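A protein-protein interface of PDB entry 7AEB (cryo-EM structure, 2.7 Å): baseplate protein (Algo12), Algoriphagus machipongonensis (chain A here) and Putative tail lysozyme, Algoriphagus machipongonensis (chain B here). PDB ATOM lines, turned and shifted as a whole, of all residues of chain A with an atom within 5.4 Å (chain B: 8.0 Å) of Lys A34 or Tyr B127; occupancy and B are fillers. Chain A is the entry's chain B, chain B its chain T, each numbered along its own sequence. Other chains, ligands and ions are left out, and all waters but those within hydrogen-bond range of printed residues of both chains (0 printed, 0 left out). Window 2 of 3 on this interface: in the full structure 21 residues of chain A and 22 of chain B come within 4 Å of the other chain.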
ATOM      1  N   GLY A  29       9.068  -0.062   9.991  1.00  0.00           N
ATOM      2  CA  GLY A  29       9.567  -1.174  10.768  1.00  0.00           C
ATOM      3  C   GLY A  29       8.529  -1.670  11.739  1.00  0.00           C
ATOM      4  O   GLY A  29       8.217  -2.861  11.766  1.00  0.00           O
ATOM      5  N   ILE A  30       7.957  -0.752  12.508  1.00  0.00           N
ATOM      6  CA  ILE A  30       6.959  -1.129  13.492  1.00  0.00           C
ATOM      7  C   ILE A  30       5.716  -1.698  12.839  1.00  0.00           C
ATOM      8  O   ILE A  30       5.143  -2.660  13.359  1.00  0.00           O
ATOM      9  CB  ILE A  30       6.644   0.032  14.439  1.00  0.00           C
ATOM     10  CG1 ILE A  30       7.902   0.267  15.287  1.00  0.00           C
ATOM     11  CG2 ILE A  30       5.455  -0.343  15.333  1.00  0.00           C
ATOM     12  CD1 ILE A  30       7.931   1.525  16.073  1.00  0.00           C
ATOM     13  N   ARG A  31       5.260  -1.113  11.732  1.00  0.00           N
ATOM     14  CA  ARG A  31       4.099  -1.666  11.045  1.00  0.00           C
ATOM     15  C   ARG A  31       4.325  -3.117  10.656  1.00  0.00           C
ATOM     16  O   ARG A  31       3.455  -3.960  10.889  1.00  0.00           O
ATOM     17  CB  ARG A  31       3.773  -0.854   9.803  1.00  0.00           C
ATOM     18  CG  ARG A  31       2.576  -1.360   9.039  1.00  0.00           C
ATOM     19  CD  ARG A  31       2.191  -0.470   7.886  1.00  0.00           C
ATOM     20  NE  ARG A  31       3.172  -0.399   6.789  1.00  0.00           N
ATOM     21  CZ  ARG A  31       3.342  -1.324   5.817  1.00  0.00           C
ATOM     22  NH1 ARG A  31       2.646  -2.457   5.777  1.00  0.00           N
ATOM     23  NH2 ARG A  31       4.230  -1.101   4.862  1.00  0.00           N
ATOM     24  N   TYR A  32       5.503  -3.436  10.119  1.00  0.00           N
ATOM     25  CA  TYR A  32       5.781  -4.812   9.739  1.00  0.00           C
ATOM     26  C   TYR A  32       5.786  -5.739  10.944  1.00  0.00           C
ATOM     27  O   TYR A  32       5.260  -6.850  10.861  1.00  0.00           O
ATOM     28  CB  TYR A  32       7.115  -4.916   9.016  1.00  0.00           C
ATOM     29  CG  TYR A  32       7.136  -4.281   7.668  1.00  0.00           C
ATOM     30  CD1 TYR A  32       8.092  -3.348   7.361  1.00  0.00           C
ATOM     31  CD2 TYR A  32       6.212  -4.613   6.719  1.00  0.00           C
ATOM     32  CE1 TYR A  32       8.119  -2.749   6.150  1.00  0.00           C
ATOM     33  CE2 TYR A  32       6.242  -4.014   5.500  1.00  0.00           C
ATOM     34  CZ  TYR A  32       7.193  -3.088   5.220  1.00  0.00           C
ATOM     35  OH  TYR A  32       7.217  -2.491   3.992  1.00  0.00           O
ATOM     36  N   ILE A  33       6.341  -5.280  12.069  1.00  0.00           N
ATOM     37  CA  ILE A  33       6.385  -6.093  13.279  1.00  0.00           C
ATOM     38  C   ILE A  33       4.999  -6.457  13.738  1.00  0.00           C
ATOM     39  O   ILE A  33       4.751  -7.607  14.084  1.00  0.00           O
ATOM     40  CB  ILE A  33       7.118  -5.375  14.422  1.00  0.00           C
ATOM     41  CG1 ILE A  33       8.600  -5.270  14.095  1.00  0.00           C
ATOM     42  CG2 ILE A  33       6.882  -6.112  15.768  1.00  0.00           C
ATOM     43  CD1 ILE A  33       9.374  -4.315  14.974  1.00  0.00           C
ATOM     44  N   LYS A  34       4.073  -5.510  13.774  1.00  0.00           N
ATOM     45  CA  LYS A  34       2.727  -5.847  14.220  1.00  0.00           C
ATOM     46  C   LYS A  34       2.064  -6.841  13.323  1.00  0.00           C
ATOM     47  O   LYS A  34       1.402  -7.742  13.796  1.00  0.00           O
ATOM     48  CB  LYS A  34       1.824  -4.644  14.230  1.00  0.00           C
ATOM     49  CG  LYS A  34       2.149  -3.615  15.250  1.00  0.00           C
ATOM     50  CD  LYS A  34       1.050  -2.579  15.306  1.00  0.00           C
ATOM     51  CE  LYS A  34       0.997  -1.751  14.041  1.00  0.00           C
ATOM     52  NZ  LYS A  34       0.015  -0.633  14.072  1.00  0.00           N
ATOM     53  N   GLU A  35       2.210  -6.675  12.025  1.00  0.00           N
ATOM     54  CA  GLU A  35       1.564  -7.574  11.083  1.00  0.00           C
ATOM     55  C   GLU A  35       2.053  -9.003  11.209  1.00  0.00           C
ATOM     56  O   GLU A  35       1.267  -9.943  11.087  1.00  0.00           O
ATOM     57  CB  GLU A  35       1.811  -7.076   9.668  1.00  0.00           C
ATOM     58  CG  GLU A  35       1.081  -5.785   9.343  1.00  0.00           C
ATOM     59  CD  GLU A  35       1.468  -5.207   8.012  1.00  0.00           C
ATOM     60  OE1 GLU A  35       2.293  -5.803   7.348  1.00  0.00           O
ATOM     61  OE2 GLU A  35       0.961  -4.148   7.651  1.00  0.00           O
ATOM     62  N   LEU A  36       3.334  -9.181  11.466  1.00  0.00           N
ATOM     63  CA  LEU A  36       3.910 -10.507  11.558  1.00  0.00           C
ATOM     64  C   LEU A  36       3.907 -11.145  12.944  1.00  0.00           C
ATOM     65  O   LEU A  36       3.706 -12.357  13.049  1.00  0.00           O
ATOM     66  CB  LEU A  36       5.351 -10.436  11.090  1.00  0.00           C
ATOM     67  CG  LEU A  36       5.591 -10.037   9.641  1.00  0.00           C
ATOM     68  CD1 LEU A  36       7.053  -9.819   9.450  1.00  0.00           C
ATOM     69  CD2 LEU A  36       5.112 -11.116   8.702  1.00  0.00           C
ATOM     70  N   GLY A  37       4.186 -10.391  14.007  1.00  0.00           N
ATOM     71  CA  GLY A  37       4.361 -11.005  15.314  1.00  0.00           C
ATOM     72  C   GLY A  37       3.588 -10.482  16.520  1.00  0.00           C
ATOM     73  O   GLY A  37       3.952 -10.843  17.644  1.00  0.00           O
ATOM     74  N   SER A  38       2.495  -9.727  16.331  1.00  0.00           N
ATOM     75  CA  SER A  38       1.758  -9.149  17.462  1.00  0.00           C
ATOM     76  C   SER A  38       1.174 -10.164  18.438  1.00  0.00           C
ATOM     77  O   SER A  38       0.807  -9.798  19.549  1.00  0.00           O
ATOM     78  CB  SER A  38       0.639  -8.278  16.957  1.00  0.00           C
ATOM     79  OG  SER A  38      -0.339  -9.049  16.321  1.00  0.00           O
ATOM     80  N   THR A  42       4.182  -7.537  21.919  1.00  0.00           N
ATOM     81  CA  THR A  42       3.251  -6.412  21.985  1.00  0.00           C
ATOM     82  C   THR A  42       3.809  -5.154  22.653  1.00  0.00           C
ATOM     83  O   THR A  42       3.249  -4.070  22.489  1.00  0.00           O
ATOM     84  CB  THR A  42       1.991  -6.827  22.740  1.00  0.00           C
ATOM     85  OG1 THR A  42       2.348  -7.180  24.075  1.00  0.00           O
ATOM     86  CG2 THR A  42       1.372  -8.005  22.071  1.00  0.00           C
ATOM     87  N   ASP A  43       4.879  -5.259  23.406  1.00  0.00           N
ATOM     88  CA  ASP A  43       5.456  -4.138  24.128  1.00  0.00           C
ATOM     89  C   ASP A  43       6.395  -3.389  23.194  1.00  0.00           C
ATOM     90  O   ASP A  43       7.505  -3.838  22.977  1.00  0.00           O
ATOM     91  CB  ASP A  43       6.200  -4.739  25.317  1.00  0.00           C
ATOM     92  CG  ASP A  43       7.023  -3.757  26.091  1.00  0.00           C
ATOM     93  OD1 ASP A  43       7.220  -2.625  25.690  1.00  0.00           O
ATOM     94  OD2 ASP A  43       7.539  -4.125  27.143  1.00  0.00           O
ATOM     95  N   TYR A  44       6.020  -2.192  22.748  1.00  0.00           N
ATOM     96  CA  TYR A  44       6.868  -1.461  21.809  1.00  0.00           C
ATOM     97  C   TYR A  44       7.456  -0.211  22.438  1.00  0.00           C
ATOM     98  O   TYR A  44       7.748   0.761  21.742  1.00  0.00           O
ATOM     99  CB  TYR A  44       6.125  -1.115  20.519  1.00  0.00           C
ATOM    100  CG  TYR A  44       5.516  -2.308  19.838  1.00  0.00           C
ATOM    101  CD1 TYR A  44       4.244  -2.230  19.395  1.00  0.00           C
ATOM    102  CD2 TYR A  44       6.196  -3.506  19.700  1.00  0.00           C
ATOM    103  CE1 TYR A  44       3.644  -3.296  18.827  1.00  0.00           C
ATOM    104  CE2 TYR A  44       5.588  -4.575  19.137  1.00  0.00           C
ATOM    105  CZ  TYR A  44       4.311  -4.462  18.703  1.00  0.00           C
ATOM    106  OH  TYR A  44       3.656  -5.531  18.169  1.00  0.00           O
ATOM    107  N   ASP B   7      -3.368  -7.404  30.437  1.00  0.00           N
ATOM    108  CA  ASP B   7      -2.743  -7.470  29.113  1.00  0.00           C
ATOM    109  C   ASP B   7      -2.210  -6.118  28.656  1.00  0.00           C
ATOM    110  O   ASP B   7      -1.591  -6.050  27.589  1.00  0.00           O
ATOM    111  CB  ASP B   7      -3.791  -7.975  28.137  1.00  0.00           C
ATOM    112  CG  ASP B   7      -4.161  -9.374  28.393  1.00  0.00           C
ATOM    113  OD1 ASP B   7      -4.858  -9.889  27.529  1.00  0.00           O
ATOM    114  OD2 ASP B   7      -3.643  -9.967  29.379  1.00  0.00           O
ATOM    115  N   PHE B   8      -2.439  -5.036  29.416  1.00  0.00           N
ATOM    116  CA  PHE B   8      -1.896  -3.737  29.021  1.00  0.00           C
ATOM    117  C   PHE B   8      -0.538  -3.455  29.629  1.00  0.00           C
ATOM    118  O   PHE B   8       0.011  -2.370  29.418  1.00  0.00           O
ATOM    119  CB  PHE B   8      -2.864  -2.554  29.298  1.00  0.00           C
ATOM    120  CG  PHE B   8      -3.264  -2.330  30.726  1.00  0.00           C
ATOM    121  CD1 PHE B   8      -2.448  -1.654  31.622  1.00  0.00           C
ATOM    122  CD2 PHE B   8      -4.526  -2.689  31.133  1.00  0.00           C
ATOM    123  CE1 PHE B   8      -2.857  -1.421  32.896  1.00  0.00           C
ATOM    124  CE2 PHE B   8      -4.936  -2.446  32.410  1.00  0.00           C
ATOM    125  CZ  PHE B   8      -4.101  -1.814  33.291  1.00  0.00           C
ATOM    126  N   GLY B  10       1.802  -5.630  28.945  1.00  0.00           N
ATOM    127  CA  GLY B  10       2.486  -6.101  27.764  1.00  0.00           C
ATOM    128  C   GLY B  10       3.516  -7.193  27.993  1.00  0.00           C
ATOM    129  O   GLY B  10       3.751  -7.665  29.108  1.00  0.00           O
ATOM    130  N   THR B  11       4.102  -7.625  26.857  1.00  0.00           N
ATOM    131  CA  THR B  11       5.099  -8.698  26.681  1.00  0.00           C
ATOM    132  C   THR B  11       6.287  -8.303  25.787  1.00  0.00           C
ATOM    133  O   THR B  11       6.063  -7.767  24.715  1.00  0.00           O
ATOM    134  CB  THR B  11       4.445  -9.903  25.976  1.00  0.00           C
ATOM    135  OG1 THR B  11       3.225 -10.253  26.621  1.00  0.00           O
ATOM    136  CG2 THR B  11       5.349 -11.103  25.975  1.00  0.00           C
ATOM    137  N   ASN B 124       1.621   4.701  27.612  1.00  0.00           N
ATOM    138  CA  ASN B 124       2.040   3.300  27.576  1.00  0.00           C
ATOM    139  C   ASN B 124       1.863   2.667  26.189  1.00  0.00           C
ATOM    140  O   ASN B 124       0.758   2.292  25.800  1.00  0.00           O
ATOM    141  CB  ASN B 124       1.249   2.552  28.629  1.00  0.00           C
ATOM    142  CG  ASN B 124       1.649   1.156  28.749  1.00  0.00           C
ATOM    143  OD1 ASN B 124       2.794   0.791  28.501  1.00  0.00           O
ATOM    144  ND2 ASN B 124       0.702   0.339  29.146  1.00  0.00           N
ATOM    145  N   MET B 125       2.931   2.530  25.420  1.00  0.00           N
ATOM    146  CA  MET B 125       2.775   2.009  24.066  1.00  0.00           C
ATOM    147  C   MET B 125       2.702   0.479  23.950  1.00  0.00           C
ATOM    148  O   MET B 125       3.612  -0.190  23.501  1.00  0.00           O
ATOM    149  CB  MET B 125       3.874   2.575  23.180  1.00  0.00           C
ATOM    150  CG  MET B 125       3.813   2.067  21.754  1.00  0.00           C
ATOM    151  SD  MET B 125       4.364   3.151  20.477  1.00  0.00           S
ATOM    152  CE  MET B 125       3.374   4.594  20.788  1.00  0.00           C
ATOM    153  N   VAL B 126       1.567  -0.077  24.343  1.00  0.00           N
ATOM    154  CA  VAL B 126       1.268  -1.506  24.248  1.00  0.00           C
ATOM    155  C   VAL B 126       0.226  -1.692  23.149  1.00  0.00           C
ATOM    156  O   VAL B 126      -0.812  -1.022  23.155  1.00  0.00           O
ATOM    157  CB  VAL B 126       0.823  -2.044  25.619  1.00  0.00           C
ATOM    158  CG1 VAL B 126       0.449  -3.502  25.566  1.00  0.00           C
ATOM    159  CG2 VAL B 126       1.967  -1.863  26.570  1.00  0.00           C
ATOM    160  N   TYR B 127       0.518  -2.583  22.193  1.00  0.00           N
ATOM    161  CA  TYR B 127      -0.148  -2.628  20.884  1.00  0.00           C
ATOM    162  C   TYR B 127      -1.680  -2.542  20.810  1.00  0.00           C
ATOM    163  O   TYR B 127      -2.178  -1.681  20.080  1.00  0.00           O
ATOM    164  CB  TYR B 127       0.321  -3.856  20.081  1.00  0.00           C
ATOM    165  CG  TYR B 127      -0.624  -4.146  18.949  1.00  0.00           C
ATOM    166  CD1 TYR B 127      -0.719  -3.290  17.862  1.00  0.00           C
ATOM    167  CD2 TYR B 127      -1.419  -5.280  18.963  1.00  0.00           C
ATOM    168  CE1 TYR B 127      -1.596  -3.533  16.872  1.00  0.00           C
ATOM    169  CE2 TYR B 127      -2.284  -5.528  17.962  1.00  0.00           C
ATOM    170  CZ  TYR B 127      -2.368  -4.660  16.919  1.00  0.00           C
ATOM    171  OH  TYR B 127      -3.246  -4.926  15.908  1.00  0.00           O
ATOM    172  N   PRO B 128      -2.488  -3.374  21.449  1.00  0.00           N
ATOM    173  CA  PRO B 128      -3.922  -3.250  21.222  1.00  0.00           C
ATOM    174  C   PRO B 128      -4.578  -2.151  22.046  1.00  0.00           C
ATOM    175  O   PRO B 128      -5.803  -2.058  22.063  1.00  0.00           O
ATOM    176  CB  PRO B 128      -4.414  -4.649  21.590  1.00  0.00           C
ATOM    177  CG  PRO B 128      -3.472  -5.074  22.666  1.00  0.00           C
ATOM    178  CD  PRO B 128      -2.164  -4.445  22.402  1.00  0.00           C
ATOM    179  N   PHE B 129      -3.802  -1.292  22.708  1.00  0.00           N
ATOM    180  CA  PHE B 129      -4.358  -0.260  23.568  1.00  0.00           C
ATOM    181  C   PHE B 129      -4.029   1.143  23.118  1.00  0.00           C
ATOM    182  O   PHE B 129      -4.943   1.962  23.023  1.00  0.00           O
ATOM    183  CB  PHE B 129      -3.878  -0.425  24.995  1.00  0.00           C
ATOM    184  CG  PHE B 129      -4.285  -1.684  25.583  1.00  0.00           C
ATOM    185  CD1 PHE B 129      -3.435  -2.752  25.557  1.00  0.00           C
ATOM    186  CD2 PHE B 129      -5.528  -1.819  26.148  1.00  0.00           C
ATOM    187  CE1 PHE B 129      -3.812  -3.935  26.080  1.00  0.00           C
ATOM    188  CE2 PHE B 129      -5.908  -3.012  26.682  1.00  0.00           C
ATOM    189  CZ  PHE B 129      -5.046  -4.072  26.650  1.00  0.00           C
ATOM    190  N   TYR B 130      -2.751   1.441  22.834  1.00  0.00           N
ATOM    191  CA  TYR B 130      -2.376   2.819  22.523  1.00  0.00           C
ATOM    192  C   TYR B 130      -3.119   3.364  21.312  1.00  0.00           C
ATOM    193  O   TYR B 130      -3.365   4.565  21.247  1.00  0.00           O
ATOM    194  CB  TYR B 130      -0.858   2.961  22.322  1.00  0.00           C
ATOM    195  CG  TYR B 130      -0.275   2.431  21.031  1.00  0.00           C
ATOM    196  CD1 TYR B 130      -0.306   3.166  19.854  1.00  0.00           C
ATOM    197  CD2 TYR B 130       0.373   1.226  21.009  1.00  0.00           C
ATOM    198  CE1 TYR B 130       0.223   2.696  18.716  1.00  0.00           C
ATOM    199  CE2 TYR B 130       0.929   0.754  19.863  1.00  0.00           C
ATOM    200  CZ  TYR B 130       0.849   1.489  18.723  1.00  0.00           C
ATOM    201  OH  TYR B 130       1.407   1.011  17.573  1.00  0.00           O
ATOM    202  N   LEU B 131      -3.569   2.488  20.420  1.00  0.00           N
ATOM    203  CA  LEU B 131      -4.248   2.929  19.214  1.00  0.00           C
ATOM    204  C   LEU B 131      -5.474   3.772  19.501  1.00  0.00           C
ATOM    205  O   LEU B 131      -5.767   4.709  18.762  1.00  0.00           O
ATOM    206  CB  LEU B 131      -4.687   1.735  18.393  1.00  0.00           C
ATOM    207  CG  LEU B 131      -3.634   0.833  17.789  1.00  0.00           C
ATOM    208  CD1 LEU B 131      -4.357  -0.273  17.057  1.00  0.00           C
ATOM    209  CD2 LEU B 131      -2.727   1.607  16.855  1.00  0.00           C
ATOM    210  N   GLU B 132      -6.214   3.445  20.555  1.00  0.00           N
ATOM    211  CA  GLU B 132      -7.354   4.269  20.851  1.00  0.00           C
ATOM    212  C   GLU B 132      -7.166   5.016  22.185  1.00  0.00           C
ATOM    213  O   GLU B 132      -7.749   6.072  22.369  1.00  0.00           O
ATOM    214  CB  GLU B 132      -8.603   3.414  20.986  1.00  0.00           C
ATOM    215  CG  GLU B 132      -9.855   4.109  20.543  1.00  0.00           C
ATOM    216  CD  GLU B 132      -9.851   4.379  19.045  1.00  0.00           C
ATOM    217  OE1 GLU B 132      -9.631   3.387  18.297  1.00  0.00           O
ATOM    218  OE2 GLU B 132     -10.072   5.516  18.612  1.00  0.00           O
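The backbone NH (N) of Thr B11 lies within hydrogen-bond range of the side-chain hydroxyl (OG1) of Thr A42, at 3.3 Å. O of Thr A42 sits at hydrogen-bond distance from N of Tyr B127 (3.1 Å). The backbone NH of Asp A43 lies within hydrogen-bond range of the backbone carbonyl oxygen of Thr B11 (3.1 Å). The backbone NH (N) of Tyr A44 sits at hydrogen-bond distance from the backbone carbonyl oxygen (O) of Met B125 (3.2 Å).
Hydrophobic or aromatic side chains of chain A within 4 Å of the printed part of chain B: Tyr A44. Along chain A the printed residues that touch a printed residue of chain B span positions 34 to 44. Hydrophobic or aromatic side chains of chain B within 4 Å of the printed part of chain A: Tyr B127. Among the printed residues, no Asp or Glu carboxylate lies within 4 Å of a Lys or Arg side-chain nitrogen of the other chain.
The backbone carbonyl oxygen (O) of Lys A34 sits close to the side-chain hydroxyl (OG) of Ser A38 (3.3 Å).
Lys A34 touches one residue of chain B. Ser A38 touches none of the printed residues of chain B. Of the printed residues of chain B, Tyr A44 touches Met B125 (3.2 Å) and Tyr B127 (3.6 Å). Of the printed residues of chain A, Gly B10 touches Thr A42. Tyr B127 touches three residues of chain A. The nearest residue of chain A that does not touch Tyr B127 is Ser A38 (4.1 Å).
Among the printed residues, pairs that only touch across the chains: Lys A34 with Tyr B127, Tyr A44 with Tyr B127, Thr A42 with Val B126 and Thr A42 with Gly B10.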
